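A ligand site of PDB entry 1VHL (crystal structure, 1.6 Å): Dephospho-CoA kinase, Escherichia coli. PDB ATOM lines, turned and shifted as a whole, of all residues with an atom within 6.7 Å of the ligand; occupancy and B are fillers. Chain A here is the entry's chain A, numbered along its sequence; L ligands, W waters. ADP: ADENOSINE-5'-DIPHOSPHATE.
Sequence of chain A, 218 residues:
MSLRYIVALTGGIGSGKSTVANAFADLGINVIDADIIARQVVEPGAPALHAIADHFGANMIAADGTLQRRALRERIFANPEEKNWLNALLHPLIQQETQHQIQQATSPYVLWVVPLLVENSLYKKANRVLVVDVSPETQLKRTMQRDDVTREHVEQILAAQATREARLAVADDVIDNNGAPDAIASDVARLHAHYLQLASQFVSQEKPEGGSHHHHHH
The side-chain amino group (NZ) of Lys 17 is in salt-bridge range of an oxygen (O3B) of the ligand.
The backbone NH (N) of Gly 14 lies within hydrogen-bond range of an oxygen (O1B) of the ligand (2.9 Å).
ND2 of Asn 177 is in hydrogen-bond range of N7 of the ligand (3.1 Å).
N of Lys 17 sits at hydrogen-bond distance from O3B of the ligand (2.7 Å).
The side-chain hydroxyl (OG) of Ser 15 lies within hydrogen-bond range of an oxygen (O3B) of the ligand.
The backbone NH (N) of Thr 19 sits at hydrogen-bond distance from an oxygen (O1A) of the ligand (3.2 Å).
The side-chain hydroxyl of Thr 19 sits at hydrogen-bond distance from an oxygen (O1A) of the ligand (3.0 Å).
The backbone NH (N) of Gly 16 lies within hydrogen-bond range of an oxygen (O3B) of the ligand, at 2.8 Å.
N of Ser 18 is in hydrogen-bond range of O2B of the ligand (3.0 Å).
The backbone NH (N) of Ser 15 is in hydrogen-bond range of an oxygen (O3B) of the ligand, 3.2 Å away.
O of Gly 179 lies within hydrogen-bond range of N6 of the ligand.
The guanidinium group (NH2) of Arg 142 lies close to a nitrogen (N1) of the ligand.
A nitrogen (N6) of the ligand sits at hydrogen-bond distance from the backbone carbonyl oxygen (O) of Asn 177 (3.5 Å).
The guanidinium group of Arg 146 lies within salt-bridge range of an oxygen (O1B) of the ligand.
The backbone carbonyl oxygen (O) of Asn 177 lies within hydrogen-bond range of the guanidinium group (NH2) of Arg 142, at 2.7 Å.
The side-chain amino group (NZ) of Lys 17 is in hydrogen-bond range of the backbone carbonyl oxygen (O) of Gly 12 (2.9 Å).
The side-chain hydroxyl (OG) of Ser 15 sits at hydrogen-bond distance from the backbone carbonyl oxygen (O) of Gly 12, at 2.7 Å.
O of Ser 15 lies within hydrogen-bond range of ND2 of Asn 177 (2.9 Å).
The side-chain amino group (NZ) of Lys 17 lies within hydrogen-bond range of the backbone carbonyl oxygen (O) of Gly 11, 2.8 Å away.
N of Pro 181 sits close to N6 of the ligand.
Gly 12 touches the ligand (O to O3B, 3.6 Å).
C of Ile 13 touches O1B of the ligand, 3.9 Å away.
Ala 180 touches the ligand (C to N6, 3.8 Å).
Hydrophobic or aromatic side chains within 4 Å of the ligand: Pro 181.
Within 4 Å of the ligand: Gly 12, Ile 13, Gly 14, Ser 15, Gly 16, Lys 17, Ser 18, Thr 19, Arg 142, Arg 146, Asn 177, Gly 179, Ala 180 and Pro 181.
Water W5 lies within hydrogen-bond range of O1B of the ligand (3.0 Å) and NH2 of Arg 146 (3.1 Å).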
ATOM      1  N   GLY A  11      -2.057 -17.796 -37.553  1.00  0.00           N
ATOM      2  CA  GLY A  11      -1.444 -18.843 -36.725  1.00  0.00           C
ATOM      3  C   GLY A  11      -1.658 -20.158 -37.463  1.00  0.00           C
ATOM      4  O   GLY A  11      -2.552 -20.259 -38.323  1.00  0.00           O
ATOM      5  N   GLY A  12      -0.855 -21.139 -37.145  1.00  0.00           N
ATOM      6  CA  GLY A  12      -1.028 -22.458 -37.821  1.00  0.00           C
ATOM      7  C   GLY A  12      -2.243 -23.173 -37.237  1.00  0.00           C
ATOM      8  O   GLY A  12      -2.892 -22.761 -36.278  1.00  0.00           O
ATOM      9  N   ILE A  13      -2.507 -24.325 -37.859  1.00  0.00           N
ATOM     10  CA  ILE A  13      -3.621 -25.151 -37.398  1.00  0.00           C
ATOM     11  C   ILE A  13      -3.464 -25.537 -35.944  1.00  0.00           C
ATOM     12  O   ILE A  13      -2.414 -25.984 -35.462  1.00  0.00           O
ATOM     13  CB  ILE A  13      -3.803 -26.393 -38.284  1.00  0.00           C
ATOM     14  CG1 ILE A  13      -5.176 -27.051 -38.006  1.00  0.00           C
ATOM     15  CG2 ILE A  13      -2.669 -27.395 -38.089  1.00  0.00           C
ATOM     16  CD1 ILE A  13      -5.471 -28.018 -39.188  1.00  0.00           C
ATOM     17  N   GLY A  14      -4.565 -25.280 -35.200  1.00  0.00           N
ATOM     18  CA  GLY A  14      -4.574 -25.665 -33.784  1.00  0.00           C
ATOM     19  C   GLY A  14      -3.819 -24.723 -32.882  1.00  0.00           C
ATOM     20  O   GLY A  14      -3.676 -24.999 -31.677  1.00  0.00           O
ATOM     21  N   SER A  15      -3.486 -23.495 -33.296  1.00  0.00           N
ATOM     22  CA  SER A  15      -2.742 -22.597 -32.424  1.00  0.00           C
ATOM     23  C   SER A  15      -3.587 -21.692 -31.544  1.00  0.00           C
ATOM     24  O   SER A  15      -3.111 -21.205 -30.512  1.00  0.00           O
ATOM     25  CB  SER A  15      -1.769 -21.718 -33.247  1.00  0.00           C
ATOM     26  OG  SER A  15      -2.514 -20.992 -34.219  1.00  0.00           O
ATOM     27  N   GLY A  16      -4.796 -21.386 -31.933  1.00  0.00           N
ATOM     28  CA  GLY A  16      -5.669 -20.542 -31.147  1.00  0.00           C
ATOM     29  C   GLY A  16      -6.328 -19.402 -31.911  1.00  0.00           C
ATOM     30  O   GLY A  16      -6.771 -18.472 -31.277  1.00  0.00           O
ATOM     31  N   LYS A  17      -6.360 -19.485 -33.251  1.00  0.00           N
ATOM     32  CA  LYS A  17      -6.981 -18.397 -33.986  1.00  0.00           C
ATOM     33  C   LYS A  17      -8.383 -18.098 -33.484  1.00  0.00           C
ATOM     34  O   LYS A  17      -8.662 -16.964 -33.122  1.00  0.00           O
ATOM     35  CB  LYS A  17      -6.988 -18.632 -35.509  1.00  0.00           C
ATOM     36  CG  LYS A  17      -5.555 -18.554 -36.063  1.00  0.00           C
ATOM     37  CD  LYS A  17      -5.527 -18.807 -37.553  1.00  0.00           C
ATOM     38  CE  LYS A  17      -5.992 -20.216 -37.892  1.00  0.00           C
ATOM     39  NZ  LYS A  17      -5.020 -21.253 -37.461  1.00  0.00           N
ATOM     40  N   SER A  18      -9.243 -19.125 -33.452  1.00  0.00           N
ATOM     41  CA  SER A  18     -10.619 -18.917 -33.046  1.00  0.00           C
ATOM     42  C   SER A  18     -10.764 -18.408 -31.634  1.00  0.00           C
ATOM     43  O   SER A  18     -11.559 -17.539 -31.298  1.00  0.00           O
ATOM     44  CB  SER A  18     -11.387 -20.246 -33.198  1.00  0.00           C
ATOM     45  OG  SER A  18     -12.733 -20.056 -32.816  1.00  0.00           O
ATOM     46  N   THR A  19      -9.987 -19.034 -30.741  1.00  0.00           N
ATOM     47  CA  THR A  19      -9.981 -18.665 -29.315  1.00  0.00           C
ATOM     48  C   THR A  19      -9.590 -17.213 -29.107  1.00  0.00           C
ATOM     49  O   THR A  19     -10.214 -16.460 -28.349  1.00  0.00           O
ATOM     50  CB  THR A  19      -8.940 -19.601 -28.658  1.00  0.00           C
ATOM     51  OG1 THR A  19      -9.383 -20.948 -28.960  1.00  0.00           O
ATOM     52  CG2 THR A  19      -8.886 -19.394 -27.165  1.00  0.00           C
ATOM     53  N   VAL A  20      -8.493 -16.834 -29.803  1.00  0.00           N
ATOM     54  CA  VAL A  20      -8.062 -15.424 -29.654  1.00  0.00           C
ATOM     55  C   VAL A  20      -9.043 -14.468 -30.236  1.00  0.00           C
ATOM     56  O   VAL A  20      -9.334 -13.378 -29.750  1.00  0.00           O
ATOM     57  CB  VAL A  20      -6.651 -15.238 -30.251  1.00  0.00           C
ATOM     58  CG1 VAL A  20      -6.232 -13.786 -30.218  1.00  0.00           C
ATOM     59  CG2 VAL A  20      -5.683 -16.129 -29.483  1.00  0.00           C
ATOM     60  N   VAL A 132      -0.724 -15.850 -33.309  1.00  0.00           N
ATOM     61  CA  VAL A 132      -0.967 -16.664 -32.095  1.00  0.00           C
ATOM     62  C   VAL A 132      -0.013 -17.842 -32.311  1.00  0.00           C
ATOM     63  O   VAL A 132      -0.084 -18.545 -33.327  1.00  0.00           O
ATOM     64  CB  VAL A 132      -2.412 -17.041 -31.874  1.00  0.00           C
ATOM     65  CG1 VAL A 132      -3.020 -17.682 -33.085  1.00  0.00           C
ATOM     66  CG2 VAL A 132      -2.469 -17.906 -30.579  1.00  0.00           C
ATOM     67  N   THR A 138       1.924 -28.836 -29.539  1.00  0.00           N
ATOM     68  CA  THR A 138       0.612 -28.334 -29.158  1.00  0.00           C
ATOM     69  C   THR A 138      -0.308 -28.372 -30.371  1.00  0.00           C
ATOM     70  O   THR A 138      -1.427 -28.855 -30.287  1.00  0.00           O
ATOM     71  CB  THR A 138       0.710 -26.890 -28.605  1.00  0.00           C
ATOM     72  OG1 THR A 138       1.382 -26.883 -27.368  1.00  0.00           O
ATOM     73  CG2 THR A 138      -0.658 -26.269 -28.433  1.00  0.00           C
ATOM     74  N   ARG A 142      -3.541 -30.571 -29.921  1.00  0.00           N
ATOM     75  CA  ARG A 142      -4.822 -29.828 -29.921  1.00  0.00           C
ATOM     76  C   ARG A 142      -5.644 -30.083 -31.150  1.00  0.00           C
ATOM     77  O   ARG A 142      -6.888 -30.187 -31.013  1.00  0.00           O
ATOM     78  CB  ARG A 142      -4.608 -28.353 -29.592  1.00  0.00           C
ATOM     79  CG  ARG A 142      -3.979 -28.090 -28.232  1.00  0.00           C
ATOM     80  CD  ARG A 142      -4.035 -26.625 -27.836  1.00  0.00           C
ATOM     81  NE  ARG A 142      -3.168 -26.302 -26.699  1.00  0.00           N
ATOM     82  CZ  ARG A 142      -2.794 -25.070 -26.369  1.00  0.00           C
ATOM     83  NH1 ARG A 142      -3.205 -24.034 -27.103  1.00  0.00           N
ATOM     84  NH2 ARG A 142      -1.998 -24.825 -25.324  1.00  0.00           N
ATOM     85  N   THR A 143      -5.072 -30.219 -32.327  1.00  0.00           N
ATOM     86  CA  THR A 143      -5.794 -30.457 -33.573  1.00  0.00           C
ATOM     87  C   THR A 143      -6.318 -31.899 -33.578  1.00  0.00           C
ATOM     88  O   THR A 143      -7.459 -32.165 -33.966  1.00  0.00           O
ATOM     89  CB  THR A 143      -4.978 -30.182 -34.831  1.00  0.00           C
ATOM     90  OG1 THR A 143      -4.500 -28.812 -34.807  1.00  0.00           O
ATOM     91  CG2 THR A 143      -5.843 -30.357 -36.079  1.00  0.00           C
ATOM     92  N   GLN A 145      -7.148 -33.772 -30.960  1.00  0.00           N
ATOM     93  CA  GLN A 145      -8.280 -33.799 -30.060  1.00  0.00           C
ATOM     94  C   GLN A 145      -9.509 -33.136 -30.673  1.00  0.00           C
ATOM     95  O   GLN A 145     -10.567 -33.753 -30.801  1.00  0.00           O
ATOM     96  CB  GLN A 145      -7.932 -33.114 -28.727  1.00  0.00           C
ATOM     97  CG  GLN A 145      -9.016 -33.306 -27.679  1.00  0.00           C
ATOM     98  CD  GLN A 145      -8.512 -33.255 -26.256  1.00  0.00           C
ATOM     99  OE1 GLN A 145      -7.567 -32.557 -25.909  1.00  0.00           O
ATOM    100  NE2 GLN A 145      -9.171 -34.014 -25.370  1.00  0.00           N
ATOM    101  N   ARG A 146      -9.366 -31.865 -31.049  1.00  0.00           N
ATOM    102  CA  ARG A 146     -10.436 -31.078 -31.604  1.00  0.00           C
ATOM    103  C   ARG A 146     -11.117 -31.677 -32.822  1.00  0.00           C
ATOM    104  O   ARG A 146     -12.346 -31.646 -32.887  1.00  0.00           O
ATOM    105  CB  ARG A 146      -9.915 -29.669 -32.012  1.00  0.00           C
ATOM    106  CG  ARG A 146     -11.019 -28.718 -32.402  1.00  0.00           C
ATOM    107  CD  ARG A 146     -10.491 -27.446 -33.037  1.00  0.00           C
ATOM    108  NE  ARG A 146      -9.944 -27.695 -34.358  1.00  0.00           N
ATOM    109  CZ  ARG A 146      -9.216 -26.854 -35.092  1.00  0.00           C
ATOM    110  NH1 ARG A 146      -8.936 -25.646 -34.637  1.00  0.00           N
ATOM    111  NH2 ARG A 146      -8.768 -27.246 -36.277  1.00  0.00           N
ATOM    112  N   ASP A 176       1.232 -15.914 -27.006  1.00  0.00           N
ATOM    113  CA  ASP A 176       1.604 -17.323 -26.752  1.00  0.00           C
ATOM    114  C   ASP A 176       0.436 -18.089 -26.191  1.00  0.00           C
ATOM    115  O   ASP A 176      -0.110 -17.755 -25.141  1.00  0.00           O
ATOM    116  CB  ASP A 176       2.829 -17.347 -25.863  1.00  0.00           C
ATOM    117  CG  ASP A 176       3.293 -18.700 -25.378  1.00  0.00           C
ATOM    118  OD1 ASP A 176       2.502 -19.657 -25.291  1.00  0.00           O
ATOM    119  OD2 ASP A 176       4.491 -18.807 -25.041  1.00  0.00           O
ATOM    120  N   ASN A 177       0.050 -19.177 -26.864  1.00  0.00           N
ATOM    121  CA  ASN A 177      -1.075 -19.963 -26.397  1.00  0.00           C
ATOM    122  C   ASN A 177      -0.651 -21.362 -25.994  1.00  0.00           C
ATOM    123  O   ASN A 177      -1.514 -22.220 -25.857  1.00  0.00           O
ATOM    124  CB  ASN A 177      -2.148 -20.000 -27.491  1.00  0.00           C
ATOM    125  CG  ASN A 177      -3.546 -20.346 -27.059  1.00  0.00           C
ATOM    126  OD1 ASN A 177      -3.913 -20.138 -25.891  1.00  0.00           O
ATOM    127  ND2 ASN A 177      -4.373 -20.882 -27.940  1.00  0.00           N
ATOM    128  N   ASN A 178       0.642 -21.676 -25.817  1.00  0.00           N
ATOM    129  CA  ASN A 178       0.871 -23.114 -25.471  1.00  0.00           C
ATOM    130  C   ASN A 178       0.941 -23.344 -23.972  1.00  0.00           C
ATOM    131  O   ASN A 178       1.359 -24.404 -23.483  1.00  0.00           O
ATOM    132  CB  ASN A 178       1.791 -23.843 -26.360  1.00  0.00           C
ATOM    133  CG  ASN A 178       3.243 -23.546 -26.488  1.00  0.00           C
ATOM    134  OD1 ASN A 178       4.009 -24.478 -26.765  1.00  0.00           O
ATOM    135  ND2 ASN A 178       3.725 -22.325 -26.326  1.00  0.00           N
ATOM    136  N   GLY A 179       0.422 -22.390 -23.207  1.00  0.00           N
ATOM    137  CA  GLY A 179       0.322 -22.423 -21.770  1.00  0.00           C
ATOM    138  C   GLY A 179      -1.176 -22.490 -21.404  1.00  0.00           C
ATOM    139  O   GLY A 179      -1.970 -23.070 -22.137  1.00  0.00           O
ATOM    140  N   ALA A 180      -1.539 -21.779 -20.342  1.00  0.00           N
ATOM    141  CA  ALA A 180      -2.908 -21.749 -19.852  1.00  0.00           C
ATOM    142  C   ALA A 180      -3.878 -20.975 -20.719  1.00  0.00           C
ATOM    143  O   ALA A 180      -3.675 -19.808 -21.054  1.00  0.00           O
ATOM    144  CB  ALA A 180      -2.927 -21.173 -18.429  1.00  0.00           C
ATOM    145  N   PRO A 181      -5.028 -21.571 -20.989  1.00  0.00           N
ATOM    146  CA  PRO A 181      -6.088 -20.970 -21.791  1.00  0.00           C
ATOM    147  C   PRO A 181      -6.535 -19.621 -21.248  1.00  0.00           C
ATOM    148  O   PRO A 181      -6.952 -18.728 -22.009  1.00  0.00           O
ATOM    149  CB  PRO A 181      -7.227 -21.971 -21.744  1.00  0.00           C
ATOM    150  CG  PRO A 181      -6.878 -22.959 -20.682  1.00  0.00           C
ATOM    151  CD  PRO A 181      -5.371 -22.966 -20.611  1.00  0.00           C
ATOM    152  N   ASP A 182      -6.486 -19.476 -19.928  1.00  0.00           N
ATOM    153  CA  ASP A 182      -6.870 -18.230 -19.300  1.00  0.00           C
ATOM    154  C   ASP A 182      -5.754 -17.226 -19.195  1.00  0.00           C
ATOM    155  O   ASP A 182      -5.898 -16.346 -18.312  1.00  0.00           O
ATOM    156  CB  ASP A 182      -7.513 -18.491 -17.931  1.00  0.00           C
ATOM    157  N   ILE A 184      -4.851 -15.881 -21.838  1.00  0.00           N
ATOM    158  CA  ILE A 184      -5.308 -15.319 -23.082  1.00  0.00           C
ATOM    159  C   ILE A 184      -6.004 -13.991 -22.844  1.00  0.00           C
ATOM    160  O   ILE A 184      -5.672 -13.022 -23.481  1.00  0.00           O
ATOM    161  CB  ILE A 184      -6.229 -16.299 -23.836  1.00  0.00           C
ATOM    162  CG1 ILE A 184      -5.433 -17.477 -24.371  1.00  0.00           C
ATOM    163  CG2 ILE A 184      -7.065 -15.657 -24.910  1.00  0.00           C
ATOM    164  CD1 ILE A 184      -4.316 -17.186 -25.344  1.00  0.00           C
HETATM  165  PB  ADP L   1      -7.116 -22.624 -34.620  1.00  0.00           P
HETATM  166  O1B ADP L   1      -6.943 -23.753 -35.607  1.00  0.00           O
HETATM  167  O2B ADP L   1      -8.389 -21.677 -34.858  1.00  0.00           O
HETATM  168  O3B ADP L   1      -5.868 -21.823 -34.523  1.00  0.00           O
HETATM  169  PA  ADP L   1      -8.310 -23.124 -32.049  1.00  0.00           P
HETATM  170  O1A ADP L   1      -8.571 -21.744 -31.770  1.00  0.00           O
HETATM  171  O2A ADP L   1      -9.658 -23.759 -32.390  1.00  0.00           O
HETATM  172  O3A ADP L   1      -7.295 -23.279 -33.223  1.00  0.00           O
HETATM  173  O5' ADP L   1      -7.630 -24.001 -30.929  1.00  0.00           O
HETATM  174  C5' ADP L   1      -7.344 -25.404 -31.238  1.00  0.00           C
HETATM  175  C4' ADP L   1      -7.942 -26.176 -30.053  1.00  0.00           C
HETATM  176  O4' ADP L   1      -7.239 -25.768 -28.874  1.00  0.00           O
HETATM  177  C3' ADP L   1      -9.415 -25.809 -29.827  1.00  0.00           C
HETATM  178  O3' ADP L   1     -10.193 -26.957 -29.498  1.00  0.00           O
HETATM  179  C2' ADP L   1      -9.411 -24.883 -28.626  1.00  0.00           C
HETATM  180  O2' ADP L   1     -10.630 -25.013 -27.860  1.00  0.00           O
HETATM  181  C1' ADP L   1      -8.191 -25.333 -27.895  1.00  0.00           C
HETATM  182  N9  ADP L   1      -7.603 -24.307 -26.993  1.00  0.00           N
HETATM  183  C8  ADP L   1      -7.401 -22.998 -27.249  1.00  0.00           C
HETATM  184  N7  ADP L   1      -6.479 -22.540 -26.377  1.00  0.00           N
HETATM  185  C5  ADP L   1      -6.097 -23.526 -25.601  1.00  0.00           C
HETATM  186  C6  ADP L   1      -5.212 -23.686 -24.559  1.00  0.00           C
HETATM  187  N6  ADP L   1      -4.464 -22.681 -24.104  1.00  0.00           N
HETATM  188  N1  ADP L   1      -5.073 -24.911 -23.972  1.00  0.00           N
HETATM  189  C2  ADP L   1      -5.782 -25.960 -24.376  1.00  0.00           C
HETATM  190  N3  ADP L   1      -6.640 -25.837 -25.377  1.00  0.00           N
HETATM  191  C4  ADP L   1      -6.812 -24.652 -25.996  1.00  0.00           C
HETATM  192  O   HOH W   1      -7.070 -28.789 -26.151  1.00  0.00           O
HETATM  193  O   HOH W   2      -4.718 -23.796 -29.319  1.00  0.00           O
HETATM  194  O   HOH W   3      -2.780 -20.433 -23.525  1.00  0.00           O
HETATM  195  O   HOH W   4     -12.122 -23.977 -32.020  1.00  0.00           O
HETATM  196  O   HOH W   5      -8.297 -24.733 -38.112  1.00  0.00           O
HETATM  197  O   HOH W   6      -9.059 -21.646 -37.550  1.00  0.00           O
